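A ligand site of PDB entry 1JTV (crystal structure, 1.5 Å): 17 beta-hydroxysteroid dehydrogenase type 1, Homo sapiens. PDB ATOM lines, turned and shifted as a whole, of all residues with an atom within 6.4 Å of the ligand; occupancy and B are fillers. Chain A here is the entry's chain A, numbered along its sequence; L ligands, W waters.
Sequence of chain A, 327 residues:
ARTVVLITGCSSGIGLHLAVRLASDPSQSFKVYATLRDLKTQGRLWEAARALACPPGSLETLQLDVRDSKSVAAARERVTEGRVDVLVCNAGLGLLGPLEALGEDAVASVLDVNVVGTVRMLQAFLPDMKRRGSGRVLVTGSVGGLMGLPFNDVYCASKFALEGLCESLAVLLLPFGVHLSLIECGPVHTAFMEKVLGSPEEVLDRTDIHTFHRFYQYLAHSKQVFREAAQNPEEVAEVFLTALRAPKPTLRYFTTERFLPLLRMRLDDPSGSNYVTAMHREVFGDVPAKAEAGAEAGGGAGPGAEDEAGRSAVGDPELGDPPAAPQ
Residues that only touch the ligand: Tyr 218, Val 143, Ser 222, Phe 259, Val 225, Phe 226, Pro 187 and Leu 149.
The nearest printed residue that does not touch the ligand is Met 279 (4.1 Å).
Water W1 lies within hydrogen-bond range of O1 of the ligand and N of Val 188.
Water W2 bridges the side-chain hydroxyl of Ser 222 (2.9 Å) and the side-chain hydroxyl of Tyr 218 (3.1 Å).
Water W4 lies within hydrogen-bond range of the backbone carbonyl oxygen of Cys 185 (2.7 Å), the side-chain hydroxyl of Ser 142 (2.9 Å) and the backbone carbonyl oxygen of Gly 186 (3.4 Å).
OH of Tyr 218 sits at hydrogen-bond distance from OD1 of Asn 152.
A ring nitrogen (ND1) of His 221 lies close to the backbone carbonyl oxygen of Glu 282, 3.4 Å away.
N of Val 143 sits at hydrogen-bond distance from O of Cys 185 (3.0 Å).
An oxygen (O2) of the ligand sits at hydrogen-bond distance from a ring nitrogen (NE2) of His 221, at 2.7 Å.
OE1 of Glu 282 lies within hydrogen-bond range of O2 of the ligand, 2.7 Å away.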
ATOM      1  N   LEU A  96      25.779  17.838  32.566  1.00  0.00           N
ATOM      2  CA  LEU A  96      24.426  17.937  32.022  1.00  0.00           C
ATOM      3  C   LEU A  96      23.439  18.390  33.081  1.00  0.00           C
ATOM      4  O   LEU A  96      23.513  17.897  34.219  1.00  0.00           O
ATOM      5  CB  LEU A  96      24.078  16.548  31.469  1.00  0.00           C
ATOM      6  CG  LEU A  96      22.874  16.324  30.579  1.00  0.00           C
ATOM      7  CD1 LEU A  96      23.041  16.930  29.199  1.00  0.00           C
ATOM      8  CD2 LEU A  96      22.629  14.808  30.436  1.00  0.00           C
ATOM      9  N   SER A 142      33.589  17.684  19.691  1.00  0.00           N
ATOM     10  CA  SER A 142      32.226  17.161  19.792  1.00  0.00           C
ATOM     11  C   SER A 142      31.315  17.945  18.854  1.00  0.00           C
ATOM     12  O   SER A 142      31.579  19.128  18.625  1.00  0.00           O
ATOM     13  CB  SER A 142      31.736  17.422  21.230  1.00  0.00           C
ATOM     14  OG  SER A 142      30.355  17.158  21.390  1.00  0.00           O
ATOM     15  N   VAL A 143      30.213  17.336  18.470  1.00  0.00           N
ATOM     16  CA  VAL A 143      29.181  18.093  17.718  1.00  0.00           C
ATOM     17  C   VAL A 143      28.677  19.183  18.659  1.00  0.00           C
ATOM     18  O   VAL A 143      28.274  20.255  18.192  1.00  0.00           O
ATOM     19  CB  VAL A 143      28.064  17.169  17.233  1.00  0.00           C
ATOM     20  CG1 VAL A 143      27.491  16.370  18.392  1.00  0.00           C
ATOM     21  CG2 VAL A 143      26.930  17.937  16.541  1.00  0.00           C
ATOM     22  N   GLY A 144      28.698  19.043  19.978  1.00  0.00           N
ATOM     23  CA  GLY A 144      28.360  20.057  20.951  1.00  0.00           C
ATOM     24  C   GLY A 144      29.326  21.256  20.980  1.00  0.00           C
ATOM     25  O   GLY A 144      29.075  22.256  21.675  1.00  0.00           O
ATOM     26  N   MET A 147      27.491  23.260  17.731  1.00  0.00           N
ATOM     27  CA  MET A 147      26.108  23.755  17.839  1.00  0.00           C
ATOM     28  C   MET A 147      25.649  23.589  19.276  1.00  0.00           C
ATOM     29  O   MET A 147      26.056  22.623  19.945  1.00  0.00           O
ATOM     30  CB  MET A 147      25.226  23.034  16.816  1.00  0.00           C
ATOM     31  CG  MET A 147      25.022  21.574  17.171  1.00  0.00           C
ATOM     32  SD  MET A 147      24.264  20.666  15.812  1.00  0.00           S
ATOM     33  CE  MET A 147      25.592  20.568  14.633  1.00  0.00           C
ATOM     34  N   LEU A 149      23.523  22.844  22.588  1.00  0.00           N
ATOM     35  CA  LEU A 149      22.548  21.782  22.958  1.00  0.00           C
ATOM     36  C   LEU A 149      21.935  22.104  24.293  1.00  0.00           C
ATOM     37  O   LEU A 149      22.623  22.421  25.262  1.00  0.00           O
ATOM     38  CB  LEU A 149      23.259  20.445  22.987  1.00  0.00           C
ATOM     39  CG  LEU A 149      24.046  20.034  21.725  1.00  0.00           C
ATOM     40  CD1 LEU A 149      24.818  18.760  22.020  1.00  0.00           C
ATOM     41  CD2 LEU A 149      23.111  19.924  20.551  1.00  0.00           C
ATOM     42  N   PRO A 150      20.604  22.043  24.414  1.00  0.00           N
ATOM     43  CA  PRO A 150      19.967  22.409  25.662  1.00  0.00           C
ATOM     44  C   PRO A 150      20.408  21.463  26.756  1.00  0.00           C
ATOM     45  O   PRO A 150      20.689  20.272  26.521  1.00  0.00           O
ATOM     46  CB  PRO A 150      18.472  22.263  25.374  1.00  0.00           C
ATOM     47  CG  PRO A 150      18.420  21.278  24.271  1.00  0.00           C
ATOM     48  CD  PRO A 150      19.641  21.580  23.400  1.00  0.00           C
ATOM     49  N   ASN A 152      23.191  21.330  28.127  1.00  0.00           N
ATOM     50  CA  ASN A 152      24.624  21.092  27.935  1.00  0.00           C
ATOM     51  C   ASN A 152      25.304  22.457  27.859  1.00  0.00           C
ATOM     52  O   ASN A 152      26.367  22.573  27.219  1.00  0.00           O
ATOM     53  CB  ASN A 152      24.860  20.386  26.604  1.00  0.00           C
ATOM     54  CG  ASN A 152      24.411  18.940  26.614  1.00  0.00           C
ATOM     55  OD1 ASN A 152      23.216  18.644  26.394  1.00  0.00           O
ATOM     56  ND2 ASN A 152      25.342  18.038  26.880  1.00  0.00           N
ATOM     57  N   TYR A 155      28.972  22.328  29.085  1.00  0.00           N
ATOM     58  CA  TYR A 155      29.698  21.396  28.263  1.00  0.00           C
ATOM     59  C   TYR A 155      29.927  21.988  26.861  1.00  0.00           C
ATOM     60  O   TYR A 155      31.067  22.037  26.374  1.00  0.00           O
ATOM     61  CB  TYR A 155      28.876  20.100  28.105  1.00  0.00           C
ATOM     62  CG  TYR A 155      29.565  19.102  27.222  1.00  0.00           C
ATOM     63  CD1 TYR A 155      30.703  18.436  27.624  1.00  0.00           C
ATOM     64  CD2 TYR A 155      29.095  18.860  25.924  1.00  0.00           C
ATOM     65  CE1 TYR A 155      31.333  17.521  26.796  1.00  0.00           C
ATOM     66  CE2 TYR A 155      29.717  17.965  25.089  1.00  0.00           C
ATOM     67  CZ  TYR A 155      30.843  17.291  25.538  1.00  0.00           C
ATOM     68  OH  TYR A 155      31.459  16.406  24.694  1.00  0.00           O
ATOM     69  N   CYS A 185      33.469  14.360  17.104  1.00  0.00           N
ATOM     70  CA  CYS A 185      32.718  13.163  17.410  1.00  0.00           C
ATOM     71  C   CYS A 185      31.255  13.433  17.721  1.00  0.00           C
ATOM     72  O   CYS A 185      30.857  14.378  18.396  1.00  0.00           O
ATOM     73  CB  CYS A 185      33.362  12.481  18.653  1.00  0.00           C
ATOM     74  SG  CYS A 185      35.088  12.036  18.467  1.00  0.00           S
ATOM     75  N   GLY A 186      30.381  12.527  17.250  1.00  0.00           N
ATOM     76  CA  GLY A 186      28.976  12.512  17.677  1.00  0.00           C
ATOM     77  C   GLY A 186      28.960  11.596  18.903  1.00  0.00           C
ATOM     78  O   GLY A 186      30.006  11.322  19.500  1.00  0.00           O
ATOM     79  N   PRO A 187      27.808  10.990  19.234  1.00  0.00           N
ATOM     80  CA  PRO A 187      27.721  10.027  20.326  1.00  0.00           C
ATOM     81  C   PRO A 187      28.551   8.800  20.053  1.00  0.00           C
ATOM     82  O   PRO A 187      28.621   8.314  18.914  1.00  0.00           O
ATOM     83  CB  PRO A 187      26.231   9.688  20.347  1.00  0.00           C
ATOM     84  CG  PRO A 187      25.751   9.948  18.957  1.00  0.00           C
ATOM     85  CD  PRO A 187      26.533  11.186  18.531  1.00  0.00           C
ATOM     86  N   VAL A 188      29.267   8.305  21.043  1.00  0.00           N
ATOM     87  CA  VAL A 188      30.154   7.157  20.951  1.00  0.00           C
ATOM     88  C   VAL A 188      29.887   6.149  22.058  1.00  0.00           C
ATOM     89  O   VAL A 188      29.849   6.525  23.228  1.00  0.00           O
ATOM     90  CB  VAL A 188      31.654   7.590  21.055  1.00  0.00           C
ATOM     91  CG1 VAL A 188      32.570   6.430  20.739  1.00  0.00           C
ATOM     92  CG2 VAL A 188      31.957   8.766  20.138  1.00  0.00           C
ATOM     93  N   TYR A 218      14.448  16.154  27.384  1.00  0.00           N
ATOM     94  CA  TYR A 218      15.789  16.141  26.768  1.00  0.00           C
ATOM     95  C   TYR A 218      16.450  14.775  26.965  1.00  0.00           C
ATOM     96  O   TYR A 218      16.971  14.166  26.018  1.00  0.00           O
ATOM     97  CB  TYR A 218      16.693  17.263  27.333  1.00  0.00           C
ATOM     98  CG  TYR A 218      18.118  17.031  26.834  1.00  0.00           C
ATOM     99  CD1 TYR A 218      18.479  17.438  25.553  1.00  0.00           C
ATOM    100  CD2 TYR A 218      18.996  16.306  27.613  1.00  0.00           C
ATOM    101  CE1 TYR A 218      19.766  17.149  25.085  1.00  0.00           C
ATOM    102  CE2 TYR A 218      20.275  16.036  27.138  1.00  0.00           C
ATOM    103  CZ  TYR A 218      20.632  16.460  25.889  1.00  0.00           C
ATOM    104  OH  TYR A 218      21.911  16.156  25.446  1.00  0.00           O
ATOM    105  N   HIS A 221      14.943  12.002  24.777  1.00  0.00           N
ATOM    106  CA  HIS A 221      15.347  12.210  23.404  1.00  0.00           C
ATOM    107  C   HIS A 221      16.803  11.791  23.225  1.00  0.00           C
ATOM    108  O   HIS A 221      17.162  11.134  22.254  1.00  0.00           O
ATOM    109  CB  HIS A 221      15.212  13.709  23.060  1.00  0.00           C
ATOM    110  CG  HIS A 221      15.845  14.052  21.750  1.00  0.00           C
ATOM    111  ND1 HIS A 221      15.286  13.738  20.539  1.00  0.00           N
ATOM    112  CD2 HIS A 221      17.023  14.667  21.494  1.00  0.00           C
ATOM    113  CE1 HIS A 221      16.094  14.153  19.569  1.00  0.00           C
ATOM    114  NE2 HIS A 221      17.149  14.724  20.120  1.00  0.00           N
ATOM    115  N   SER A 222      17.668  12.251  24.127  1.00  0.00           N
ATOM    116  CA  SER A 222      19.091  11.916  24.067  1.00  0.00           C
ATOM    117  C   SER A 222      19.335  10.422  24.092  1.00  0.00           C
ATOM    118  O   SER A 222      20.195   9.884  23.390  1.00  0.00           O
ATOM    119  CB  SER A 222      19.810  12.603  25.249  1.00  0.00           C
ATOM    120  OG  SER A 222      21.202  12.265  25.137  1.00  0.00           O
ATOM    121  N   LYS A 223      18.635   9.720  24.989  1.00  0.00           N
ATOM    122  CA  LYS A 223      18.770   8.265  25.076  1.00  0.00           C
ATOM    123  C   LYS A 223      18.322   7.626  23.770  1.00  0.00           C
ATOM    124  O   LYS A 223      19.007   6.664  23.370  1.00  0.00           O
ATOM    125  CB  LYS A 223      17.930   7.701  26.230  1.00  0.00           C
ATOM    126  CG  LYS A 223      18.485   8.125  27.570  1.00  0.00           C
ATOM    127  CD  LYS A 223      18.513   6.993  28.576  1.00  0.00           C
ATOM    128  CE  LYS A 223      19.348   7.417  29.777  1.00  0.00           C
ATOM    129  NZ  LYS A 223      19.029   6.614  30.990  1.00  0.00           N
ATOM    130  N   VAL A 225      18.418   8.943  20.695  1.00  0.00           N
ATOM    131  CA  VAL A 225      19.434   9.199  19.657  1.00  0.00           C
ATOM    132  C   VAL A 225      20.685   8.377  19.919  1.00  0.00           C
ATOM    133  O   VAL A 225      21.300   7.873  18.979  1.00  0.00           O
ATOM    134  CB  VAL A 225      19.767  10.686  19.573  1.00  0.00           C
ATOM    135  CG1 VAL A 225      20.924  10.948  18.620  1.00  0.00           C
ATOM    136  CG2 VAL A 225      18.541  11.461  19.109  1.00  0.00           C
ATOM    137  N   PHE A 226      21.133   8.267  21.161  1.00  0.00           N
ATOM    138  CA  PHE A 226      22.311   7.490  21.526  1.00  0.00           C
ATOM    139  C   PHE A 226      22.109   6.041  21.110  1.00  0.00           C
ATOM    140  O   PHE A 226      22.993   5.406  20.517  1.00  0.00           O
ATOM    141  CB  PHE A 226      22.577   7.590  23.030  1.00  0.00           C
ATOM    142  CG  PHE A 226      23.915   7.018  23.387  1.00  0.00           C
ATOM    143  CD1 PHE A 226      25.058   7.814  23.317  1.00  0.00           C
ATOM    144  CD2 PHE A 226      24.056   5.694  23.761  1.00  0.00           C
ATOM    145  CE1 PHE A 226      26.292   7.314  23.629  1.00  0.00           C
ATOM    146  CE2 PHE A 226      25.313   5.180  24.064  1.00  0.00           C
ATOM    147  CZ  PHE A 226      26.420   5.987  23.997  1.00  0.00           C
ATOM    148  N   PHE A 259      25.110  14.940  11.616  1.00  0.00           N
ATOM    149  CA  PHE A 259      24.718  16.255  12.118  1.00  0.00           C
ATOM    150  C   PHE A 259      25.119  17.392  11.196  1.00  0.00           C
ATOM    151  O   PHE A 259      24.765  18.553  11.449  1.00  0.00           O
ATOM    152  CB  PHE A 259      25.318  16.457  13.527  1.00  0.00           C
ATOM    153  CG  PHE A 259      24.919  15.328  14.460  1.00  0.00           C
ATOM    154  CD1 PHE A 259      25.811  14.320  14.773  1.00  0.00           C
ATOM    155  CD2 PHE A 259      23.638  15.273  14.979  1.00  0.00           C
ATOM    156  CE1 PHE A 259      25.426  13.277  15.604  1.00  0.00           C
ATOM    157  CE2 PHE A 259      23.247  14.240  15.801  1.00  0.00           C
ATOM    158  CZ  PHE A 259      24.140  13.241  16.125  1.00  0.00           C
ATOM    159  N   LEU A 262      22.193  19.865  10.319  1.00  0.00           N
ATOM    160  CA  LEU A 262      21.891  20.816  11.397  1.00  0.00           C
ATOM    161  C   LEU A 262      22.968  21.897  11.426  1.00  0.00           C
ATOM    162  O   LEU A 262      22.669  23.093  11.561  1.00  0.00           O
ATOM    163  CB  LEU A 262      21.791  20.146  12.761  1.00  0.00           C
ATOM    164  CG  LEU A 262      20.498  19.465  13.189  1.00  0.00           C
ATOM    165  CD1 LEU A 262      20.752  18.470  14.311  1.00  0.00           C
ATOM    166  CD2 LEU A 262      19.430  20.463  13.627  1.00  0.00           C
ATOM    167  N   MET A 279      16.396  23.184  16.524  1.00  0.00           N
ATOM    168  CA  MET A 279      16.867  22.328  17.619  1.00  0.00           C
ATOM    169  C   MET A 279      15.821  22.224  18.722  1.00  0.00           C
ATOM    170  O   MET A 279      15.690  21.142  19.317  1.00  0.00           O
ATOM    171  CB  MET A 279      18.218  22.842  18.121  1.00  0.00           C
ATOM    172  CG  MET A 279      18.895  21.961  19.158  1.00  0.00           C
ATOM    173  SD  MET A 279      19.162  20.244  18.639  1.00  0.00           S
ATOM    174  CE  MET A 279      20.385  20.461  17.361  1.00  0.00           C
ATOM    175  N   GLU A 282      13.584  19.588  17.336  1.00  0.00           N
ATOM    176  CA  GLU A 282      14.289  18.306  17.303  1.00  0.00           C
ATOM    177  C   GLU A 282      14.354  17.645  18.669  1.00  0.00           C
ATOM    178  O   GLU A 282      14.169  16.430  18.793  1.00  0.00           O
ATOM    179  CB  GLU A 282      15.676  18.570  16.722  1.00  0.00           C
ATOM    180  CG  GLU A 282      16.763  17.611  17.122  1.00  0.00           C
ATOM    181  CD  GLU A 282      17.172  16.647  16.025  1.00  0.00           C
ATOM    182  OE1 GLU A 282      17.785  15.627  16.380  1.00  0.00           O
ATOM    183  OE2 GLU A 282      16.887  16.936  14.849  1.00  0.00           O
ATOM    184  N   VAL A 283      14.611  18.405  19.738  1.00  0.00           N
ATOM    185  CA  VAL A 283      14.738  17.815  21.059  1.00  0.00           C
ATOM    186  C   VAL A 283      13.412  17.608  21.755  1.00  0.00           C
ATOM    187  O   VAL A 283      13.168  16.566  22.404  1.00  0.00           O
ATOM    188  CB  VAL A 283      15.652  18.737  21.909  1.00  0.00           C
ATOM    189  CG1 VAL A 283      15.669  18.293  23.369  1.00  0.00           C
ATOM    190  CG2 VAL A 283      17.052  18.714  21.324  1.00  0.00           C
HETATM  191  C1  LIG L   1      23.873  12.098  23.159  1.00  0.00           C
HETATM  192  C2  LIG L   1      24.911  11.677  24.208  1.00  0.00           C
HETATM  193  C3  LIG L   1      26.282  11.729  23.633  1.00  0.00           C
HETATM  194  O1  LIG L   1      27.104  10.932  24.037  1.00  0.00           O
HETATM  195  C4  LIG L   1      26.600  12.737  22.657  1.00  0.00           C
HETATM  196  C5  LIG L   1      25.658  13.596  22.159  1.00  0.00           C
HETATM  197  C6  LIG L   1      26.060  14.627  21.161  1.00  0.00           C
HETATM  198  C7  LIG L   1      25.030  14.979  20.109  1.00  0.00           C
HETATM  199  C8  LIG L   1      23.620  15.052  20.677  1.00  0.00           C
HETATM  200  C9  LIG L   1      23.242  13.773  21.409  1.00  0.00           C
HETATM  201  C10 LIG L   1      24.168  13.507  22.597  1.00  0.00           C
HETATM  202  C11 LIG L   1      21.780  13.683  21.922  1.00  0.00           C
HETATM  203  C12 LIG L   1      20.810  13.965  20.772  1.00  0.00           C
HETATM  204  C13 LIG L   1      21.127  15.297  20.095  1.00  0.00           C
HETATM  205  C14 LIG L   1      22.572  15.258  19.588  1.00  0.00           C
HETATM  206  C15 LIG L   1      22.745  16.443  18.656  1.00  0.00           C
HETATM  207  C16 LIG L   1      21.362  16.558  17.984  1.00  0.00           C
HETATM  208  C17 LIG L   1      20.462  15.502  18.700  1.00  0.00           C
HETATM  209  O2  LIG L   1      19.086  15.887  18.688  1.00  0.00           O
HETATM  210  C18 LIG L   1      20.825  16.489  21.034  1.00  0.00           C
HETATM  211  C19 LIG L   1      23.958  14.607  23.651  1.00  0.00           C
HETATM  212  O   HOH W   1      29.528  10.169  23.351  1.00  0.00           O
HETATM  213  O   HOH W   2      23.152  13.686  26.813  1.00  0.00           O
HETATM  214  O   HOH W   3      25.939  15.783  25.487  1.00  0.00           O
HETATM  215  O   HOH W   4      29.498  14.460  20.764  1.00  0.00           O
